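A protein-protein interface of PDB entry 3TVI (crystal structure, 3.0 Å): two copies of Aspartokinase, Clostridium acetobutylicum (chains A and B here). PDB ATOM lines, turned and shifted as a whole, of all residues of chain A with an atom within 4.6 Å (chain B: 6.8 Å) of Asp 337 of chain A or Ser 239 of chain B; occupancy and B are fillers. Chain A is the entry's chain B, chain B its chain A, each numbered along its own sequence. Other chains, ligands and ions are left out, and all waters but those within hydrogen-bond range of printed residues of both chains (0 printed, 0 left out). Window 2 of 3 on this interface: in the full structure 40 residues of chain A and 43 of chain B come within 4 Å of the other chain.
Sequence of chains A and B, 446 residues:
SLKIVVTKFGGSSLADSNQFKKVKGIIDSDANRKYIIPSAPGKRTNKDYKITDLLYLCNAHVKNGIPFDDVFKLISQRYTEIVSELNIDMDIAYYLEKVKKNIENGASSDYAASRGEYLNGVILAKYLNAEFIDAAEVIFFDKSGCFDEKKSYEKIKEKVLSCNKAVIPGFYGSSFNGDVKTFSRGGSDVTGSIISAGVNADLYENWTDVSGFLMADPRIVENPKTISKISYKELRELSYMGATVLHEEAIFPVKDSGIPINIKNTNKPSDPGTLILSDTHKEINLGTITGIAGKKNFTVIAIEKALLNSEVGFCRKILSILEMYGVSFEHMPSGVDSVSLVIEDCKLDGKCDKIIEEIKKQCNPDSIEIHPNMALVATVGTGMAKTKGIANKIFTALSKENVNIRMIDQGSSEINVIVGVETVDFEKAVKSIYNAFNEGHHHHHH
The backbone NH (N) of Val 336 of chain A is in hydrogen-bond range of the side-chain carboxylate (OE1) of Glu 237 of chain B, 2.9 Å away.
The side-chain hydroxyl (OG) of Ser 338 of chain A is in hydrogen-bond range of the side-chain carboxylate (OE2) of Glu 237 of chain B, 3.1 Å away.
NH1 of Arg 236 of chain B lies within salt-bridge range of OE2 of Glu 237 of chain B (3.0 Å).
The side-chain amide nitrogen of Asn 416 of chain B is in hydrogen-bond range of the side-chain carboxylate of Glu 237 of chain B (2.8 Å).
The backbone NH (N) of Lys 305 of chain A is in hydrogen-bond range of the backbone carbonyl oxygen (O) of Asp 337 of chain A (3.1 Å).
N of Leu 307 of chain A sits at hydrogen-bond distance from OD2 of Asp 337 of chain A.
Among the printed residues, pairs that only touch across the chains: Ala 306 of chain A with Glu 248 of chain B (3.2 Å), Gly 335 of chain A with Glu 237 of chain B (3.8 Å), Val 336 of chain A with Ser 239 of chain B (3.3 Å), Val 336 of chain A with Asn 416 of chain B (3.6 Å), Asp 337 of chain A with Arg 236 of chain B (3.5 Å), Asp 337 of chain A with Ser 239 of chain B (3.98 Å) and Ser 338 of chain A with Arg 236 of chain B (3.4 Å).
Asp 337 of chain A touches just these residues of chain B: Arg 236 (3.5 Å) and Ser 239 (3.98 Å).
Of chain A, only Val 336 and Asp 337 come within 4 Å of Ser 239 of chain B.
Printed residues of chain B within 4 Å of Val 336 of chain A: Glu 237, Ser 239 and Asn 416.
Of the printed residues of chain A, Asn 416 of chain B touches Val 336.
Of the printed residues of chain A, Glu 237 of chain B touches Gly 335, Val 336 and Ser 338.
Of the printed residues of chain A, Glu 248 of chain B touches Ala 306.
Of the printed residues of chain B, Gly 335 of chain A touches Glu 237 (3.8 Å).
Ala 293 of chain B touches none of the printed residues of chain A.
The nearest printed residue of chain A that does not touch Ser 239 of chain B is Leu 307 of chain A (5.8 Å).
The nearest printed residue of chain B that does not touch Gly 335 of chain A is Asn 416 of chain B (4.4 Å).
Hydrophobic or aromatic side chains of chain A that line the printed part of chain B: Ala 306 and Val 336.
Along chain A the printed residues that touch a printed residue of chain B span positions 306 to 338.
Among the printed residues, 9 pairs touch across the chains.
Among the printed residues, no Asp or Glu carboxylate lies within 4 Å of a Lys or Arg side-chain nitrogen of the other chain.
No position is printed for both chains.
Of the 9 pairs that touch across the chains among the printed residues, none has its exchanged pair printed and touching as well.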
ATOM      1  N   GLU A 304     -15.627  10.043   7.537  1.00  0.00           N
ATOM      2  CA  GLU A 304     -16.542   8.898   7.606  1.00  0.00           C
ATOM      3  C   GLU A 304     -16.155   8.007   8.786  1.00  0.00           C
ATOM      4  O   GLU A 304     -14.983   7.695   8.963  1.00  0.00           O
ATOM      5  CB  GLU A 304     -16.496   8.091   6.302  1.00  0.00           C
ATOM      6  N   LYS A 305     -17.133   7.608   9.595  1.00  0.00           N
ATOM      7  CA  LYS A 305     -16.868   6.785  10.776  1.00  0.00           C
ATOM      8  C   LYS A 305     -18.052   5.871  11.114  1.00  0.00           C
ATOM      9  O   LYS A 305     -19.190   6.319  11.203  1.00  0.00           O
ATOM     10  CB  LYS A 305     -16.531   7.675  11.973  1.00  0.00           C
ATOM     11  N   ALA A 306     -17.762   4.591  11.322  1.00  0.00           N
ATOM     12  CA  ALA A 306     -18.791   3.558  11.496  1.00  0.00           C
ATOM     13  C   ALA A 306     -19.642   3.778  12.739  1.00  0.00           C
ATOM     14  O   ALA A 306     -19.140   3.675  13.855  1.00  0.00           O
ATOM     15  CB  ALA A 306     -18.136   2.187  11.572  1.00  0.00           C
ATOM     16  N   LEU A 307     -20.932   4.035  12.538  1.00  0.00           N
ATOM     17  CA  LEU A 307     -21.846   4.418  13.627  1.00  0.00           C
ATOM     18  C   LEU A 307     -21.343   5.639  14.417  1.00  0.00           C
ATOM     19  O   LEU A 307     -21.345   5.632  15.648  1.00  0.00           O
ATOM     20  CB  LEU A 307     -22.116   3.233  14.568  1.00  0.00           C
ATOM     21  CG  LEU A 307     -23.013   2.127  14.005  1.00  0.00           C
ATOM     22  CD1 LEU A 307     -22.890   0.839  14.811  1.00  0.00           C
ATOM     23  CD2 LEU A 307     -24.462   2.598  13.953  1.00  0.00           C
ATOM     24  N   LEU A 308     -20.919   6.685  13.704  1.00  0.00           N
ATOM     25  CA  LEU A 308     -20.506   7.941  14.341  1.00  0.00           C
ATOM     26  C   LEU A 308     -21.657   8.559  15.122  1.00  0.00           C
ATOM     27  O   LEU A 308     -21.432   9.296  16.079  1.00  0.00           O
ATOM     28  CB  LEU A 308     -20.003   8.953  13.303  1.00  0.00           C
ATOM     29  N   ASN A 309     -22.885   8.248  14.702  1.00  0.00           N
ATOM     30  CA  ASN A 309     -24.099   8.788  15.317  1.00  0.00           C
ATOM     31  C   ASN A 309     -24.424   8.222  16.701  1.00  0.00           C
ATOM     32  O   ASN A 309     -25.096   8.881  17.491  1.00  0.00           O
ATOM     33  CB  ASN A 309     -25.297   8.557  14.389  1.00  0.00           C
ATOM     34  N   GLY A 335     -23.688  14.015   8.397  1.00  0.00           N
ATOM     35  CA  GLY A 335     -24.503  13.119   7.600  1.00  0.00           C
ATOM     36  C   GLY A 335     -25.183  12.117   8.504  1.00  0.00           C
ATOM     37  O   GLY A 335     -25.662  12.470   9.591  1.00  0.00           O
ATOM     38  N   VAL A 336     -25.216  10.863   8.059  1.00  0.00           N
ATOM     39  CA  VAL A 336     -25.834   9.792   8.827  1.00  0.00           C
ATOM     40  C   VAL A 336     -24.771   9.065   9.670  1.00  0.00           C
ATOM     41  O   VAL A 336     -24.898   8.998  10.902  1.00  0.00           O
ATOM     42  CB  VAL A 336     -26.637   8.853   7.910  1.00  0.00           C
ATOM     43  CG1 VAL A 336     -27.442   7.854   8.727  1.00  0.00           C
ATOM     44  CG2 VAL A 336     -27.567   9.682   7.040  1.00  0.00           C
ATOM     45  N   ASP A 337     -23.718   8.554   9.034  1.00  0.00           N
ATOM     46  CA  ASP A 337     -22.562   8.055   9.791  1.00  0.00           C
ATOM     47  C   ASP A 337     -21.289   8.785   9.365  1.00  0.00           C
ATOM     48  O   ASP A 337     -20.202   8.217   9.363  1.00  0.00           O
ATOM     49  CB  ASP A 337     -22.422   6.528   9.653  1.00  0.00           C
ATOM     50  CG  ASP A 337     -23.328   5.744  10.629  1.00  0.00           C
ATOM     51  OD1 ASP A 337     -23.842   6.342  11.607  1.00  0.00           O
ATOM     52  OD2 ASP A 337     -23.514   4.515  10.420  1.00  0.00           O
ATOM     53  N   SER A 338     -21.438  10.062   9.023  1.00  0.00           N
ATOM     54  CA  SER A 338     -20.314  10.903   8.635  1.00  0.00           C
ATOM     55  C   SER A 338     -20.469  12.324   9.161  1.00  0.00           C
ATOM     56  O   SER A 338     -21.549  12.738   9.580  1.00  0.00           O
ATOM     57  CB  SER A 338     -20.168  10.940   7.114  1.00  0.00           C
ATOM     58  OG  SER A 338     -21.376  11.337   6.482  1.00  0.00           O
ATOM     59  N   GLU B 234     -22.615   4.262   0.164  1.00  0.00           N
ATOM     60  CA  GLU B 234     -24.042   4.523   0.167  1.00  0.00           C
ATOM     61  C   GLU B 234     -24.679   3.798   1.335  1.00  0.00           C
ATOM     62  O   GLU B 234     -25.295   4.425   2.179  1.00  0.00           O
ATOM     63  CB  GLU B 234     -24.676   4.056  -1.142  1.00  0.00           C
ATOM     64  CG  GLU B 234     -24.370   4.967  -2.318  1.00  0.00           C
ATOM     65  CD  GLU B 234     -24.672   4.344  -3.669  1.00  0.00           C
ATOM     66  OE1 GLU B 234     -24.409   3.137  -3.850  1.00  0.00           O
ATOM     67  OE2 GLU B 234     -25.145   5.074  -4.568  1.00  0.00           O
ATOM     68  N   LEU B 235     -24.507   2.478   1.387  1.00  0.00           N
ATOM     69  CA  LEU B 235     -25.138   1.627   2.407  1.00  0.00           C
ATOM     70  C   LEU B 235     -25.048   2.240   3.790  1.00  0.00           C
ATOM     71  O   LEU B 235     -26.051   2.352   4.498  1.00  0.00           O
ATOM     72  CB  LEU B 235     -24.476   0.245   2.440  1.00  0.00           C
ATOM     73  CG  LEU B 235     -24.994  -0.745   3.501  1.00  0.00           C
ATOM     74  CD1 LEU B 235     -26.474  -1.049   3.301  1.00  0.00           C
ATOM     75  CD2 LEU B 235     -24.179  -2.030   3.480  1.00  0.00           C
ATOM     76  N   ARG B 236     -23.830   2.622   4.163  1.00  0.00           N
ATOM     77  CA  ARG B 236     -23.582   3.293   5.424  1.00  0.00           C
ATOM     78  C   ARG B 236     -24.477   4.516   5.498  1.00  0.00           C
ATOM     79  O   ARG B 236     -25.313   4.654   6.396  1.00  0.00           O
ATOM     80  CB  ARG B 236     -22.114   3.704   5.507  1.00  0.00           C
ATOM     81  CG  ARG B 236     -21.781   4.661   6.639  1.00  0.00           C
ATOM     82  CD  ARG B 236     -20.324   5.128   6.581  1.00  0.00           C
ATOM     83  NE  ARG B 236     -19.982   5.883   5.367  1.00  0.00           N
ATOM     84  CZ  ARG B 236     -20.340   7.142   5.115  1.00  0.00           C
ATOM     85  NH1 ARG B 236     -21.074   7.836   5.977  1.00  0.00           N
ATOM     86  NH2 ARG B 236     -19.966   7.711   3.979  1.00  0.00           N
ATOM     87  N   GLU B 237     -24.314   5.384   4.508  1.00  0.00           N
ATOM     88  CA  GLU B 237     -25.018   6.662   4.457  1.00  0.00           C
ATOM     89  C   GLU B 237     -26.550   6.478   4.419  1.00  0.00           C
ATOM     90  O   GLU B 237     -27.286   7.415   4.718  1.00  0.00           O
ATOM     91  CB  GLU B 237     -24.505   7.460   3.246  1.00  0.00           C
ATOM     92  CG  GLU B 237     -24.715   8.952   3.304  1.00  0.00           C
ATOM     93  CD  GLU B 237     -23.860   9.632   4.355  1.00  0.00           C
ATOM     94  OE1 GLU B 237     -24.428  10.083   5.367  1.00  0.00           O
ATOM     95  OE2 GLU B 237     -22.628   9.721   4.179  1.00  0.00           O
ATOM     96  N   LEU B 238     -27.016   5.275   4.068  1.00  0.00           N
ATOM     97  CA  LEU B 238     -28.440   4.933   4.107  1.00  0.00           C
ATOM     98  C   LEU B 238     -28.791   4.052   5.307  1.00  0.00           C
ATOM     99  O   LEU B 238     -29.794   3.339   5.279  1.00  0.00           O
ATOM    100  CB  LEU B 238     -28.869   4.237   2.802  1.00  0.00           C
ATOM    101  CG  LEU B 238     -29.634   5.091   1.785  1.00  0.00           C
ATOM    102  CD1 LEU B 238     -29.626   4.462   0.408  1.00  0.00           C
ATOM    103  CD2 LEU B 238     -31.064   5.338   2.223  1.00  0.00           C
ATOM    104  N   SER B 239     -28.008   4.125   6.384  1.00  0.00           N
ATOM    105  CA  SER B 239     -28.231   3.249   7.546  1.00  0.00           C
ATOM    106  C   SER B 239     -29.597   3.396   8.236  1.00  0.00           C
ATOM    107  O   SER B 239     -29.966   2.542   9.038  1.00  0.00           O
ATOM    108  CB  SER B 239     -27.130   3.428   8.591  1.00  0.00           C
ATOM    109  OG  SER B 239     -27.340   4.609   9.338  1.00  0.00           O
ATOM    110  N   TYR B 240     -30.347   4.454   7.932  1.00  0.00           N
ATOM    111  CA  TYR B 240     -31.696   4.621   8.496  1.00  0.00           C
ATOM    112  C   TYR B 240     -32.691   3.512   8.124  1.00  0.00           C
ATOM    113  O   TYR B 240     -33.804   3.499   8.654  1.00  0.00           O
ATOM    114  CB  TYR B 240     -32.319   5.970   8.087  1.00  0.00           C
ATOM    115  CG  TYR B 240     -31.793   7.203   8.804  1.00  0.00           C
ATOM    116  CD1 TYR B 240     -31.461   7.176  10.155  1.00  0.00           C
ATOM    117  CD2 TYR B 240     -31.671   8.417   8.128  1.00  0.00           C
ATOM    118  CE1 TYR B 240     -30.993   8.311  10.798  1.00  0.00           C
ATOM    119  CE2 TYR B 240     -31.204   9.556   8.766  1.00  0.00           C
ATOM    120  CZ  TYR B 240     -30.867   9.496  10.100  1.00  0.00           C
ATOM    121  OH  TYR B 240     -30.405  10.618  10.740  1.00  0.00           O
ATOM    122  N   MET B 241     -32.312   2.603   7.225  1.00  0.00           N
ATOM    123  CA  MET B 241     -33.233   1.553   6.747  1.00  0.00           C
ATOM    124  C   MET B 241     -33.482   0.422   7.729  1.00  0.00           C
ATOM    125  O   MET B 241     -32.723   0.203   8.679  1.00  0.00           O
ATOM    126  CB  MET B 241     -32.696   0.960   5.452  1.00  0.00           C
ATOM    127  CG  MET B 241     -32.748   1.965   4.308  1.00  0.00           C
ATOM    128  SD  MET B 241     -31.869   1.190   2.715  1.00  0.00           S
ATOM    129  CE  MET B 241     -33.317   1.701   1.482  1.00  0.00           C
ATOM    130  N   LEU B 246     -27.779  -4.762   6.625  1.00  0.00           N
ATOM    131  CA  LEU B 246     -27.464  -3.447   7.165  1.00  0.00           C
ATOM    132  C   LEU B 246     -26.329  -3.565   8.187  1.00  0.00           C
ATOM    133  O   LEU B 246     -26.562  -3.957   9.333  1.00  0.00           O
ATOM    134  CB  LEU B 246     -28.719  -2.842   7.799  1.00  0.00           C
ATOM    135  CG  LEU B 246     -28.767  -1.319   7.914  1.00  0.00           C
ATOM    136  CD1 LEU B 246     -28.962  -0.687   6.546  1.00  0.00           C
ATOM    137  CD2 LEU B 246     -29.878  -0.893   8.868  1.00  0.00           C
ATOM    138  N   GLU B 248     -21.723  -2.422   8.990  1.00  0.00           N
ATOM    139  CA  GLU B 248     -20.388  -1.935   8.587  1.00  0.00           C
ATOM    140  C   GLU B 248     -19.261  -2.748   9.241  1.00  0.00           C
ATOM    141  O   GLU B 248     -18.339  -3.211   8.560  1.00  0.00           O
ATOM    142  CB  GLU B 248     -20.238  -0.442   8.916  1.00  0.00           C
ATOM    143  CG  GLU B 248     -18.825   0.042   9.263  1.00  0.00           C
ATOM    144  CD  GLU B 248     -17.780  -0.219   8.184  1.00  0.00           C
ATOM    145  OE1 GLU B 248     -17.961   0.265   7.047  1.00  0.00           O
ATOM    146  OE2 GLU B 248     -16.762  -0.885   8.479  1.00  0.00           O
ATOM    147  N   ALA B 293     -34.212   7.343   2.917  1.00  0.00           N
ATOM    148  CA  ALA B 293     -34.464   6.771   4.245  1.00  0.00           C
ATOM    149  C   ALA B 293     -34.565   7.859   5.296  1.00  0.00           C
ATOM    150  O   ALA B 293     -33.863   8.867   5.211  1.00  0.00           O
ATOM    151  CB  ALA B 293     -33.356   5.805   4.610  1.00  0.00           C
ATOM    152  N   ASN B 416     -25.163  12.552  -0.429  1.00  0.00           N
ATOM    153  CA  ASN B 416     -26.229  12.598   0.570  1.00  0.00           C
ATOM    154  C   ASN B 416     -26.692  14.012   0.902  1.00  0.00           C
ATOM    155  O   ASN B 416     -25.886  14.852   1.301  1.00  0.00           O
ATOM    156  CB  ASN B 416     -25.755  11.924   1.856  1.00  0.00           C
ATOM    157  CG  ASN B 416     -26.886  11.679   2.839  1.00  0.00           C
ATOM    158  OD1 ASN B 416     -28.061  11.696   2.467  1.00  0.00           O
ATOM    159  ND2 ASN B 416     -26.537  11.435   4.101  1.00  0.00           N
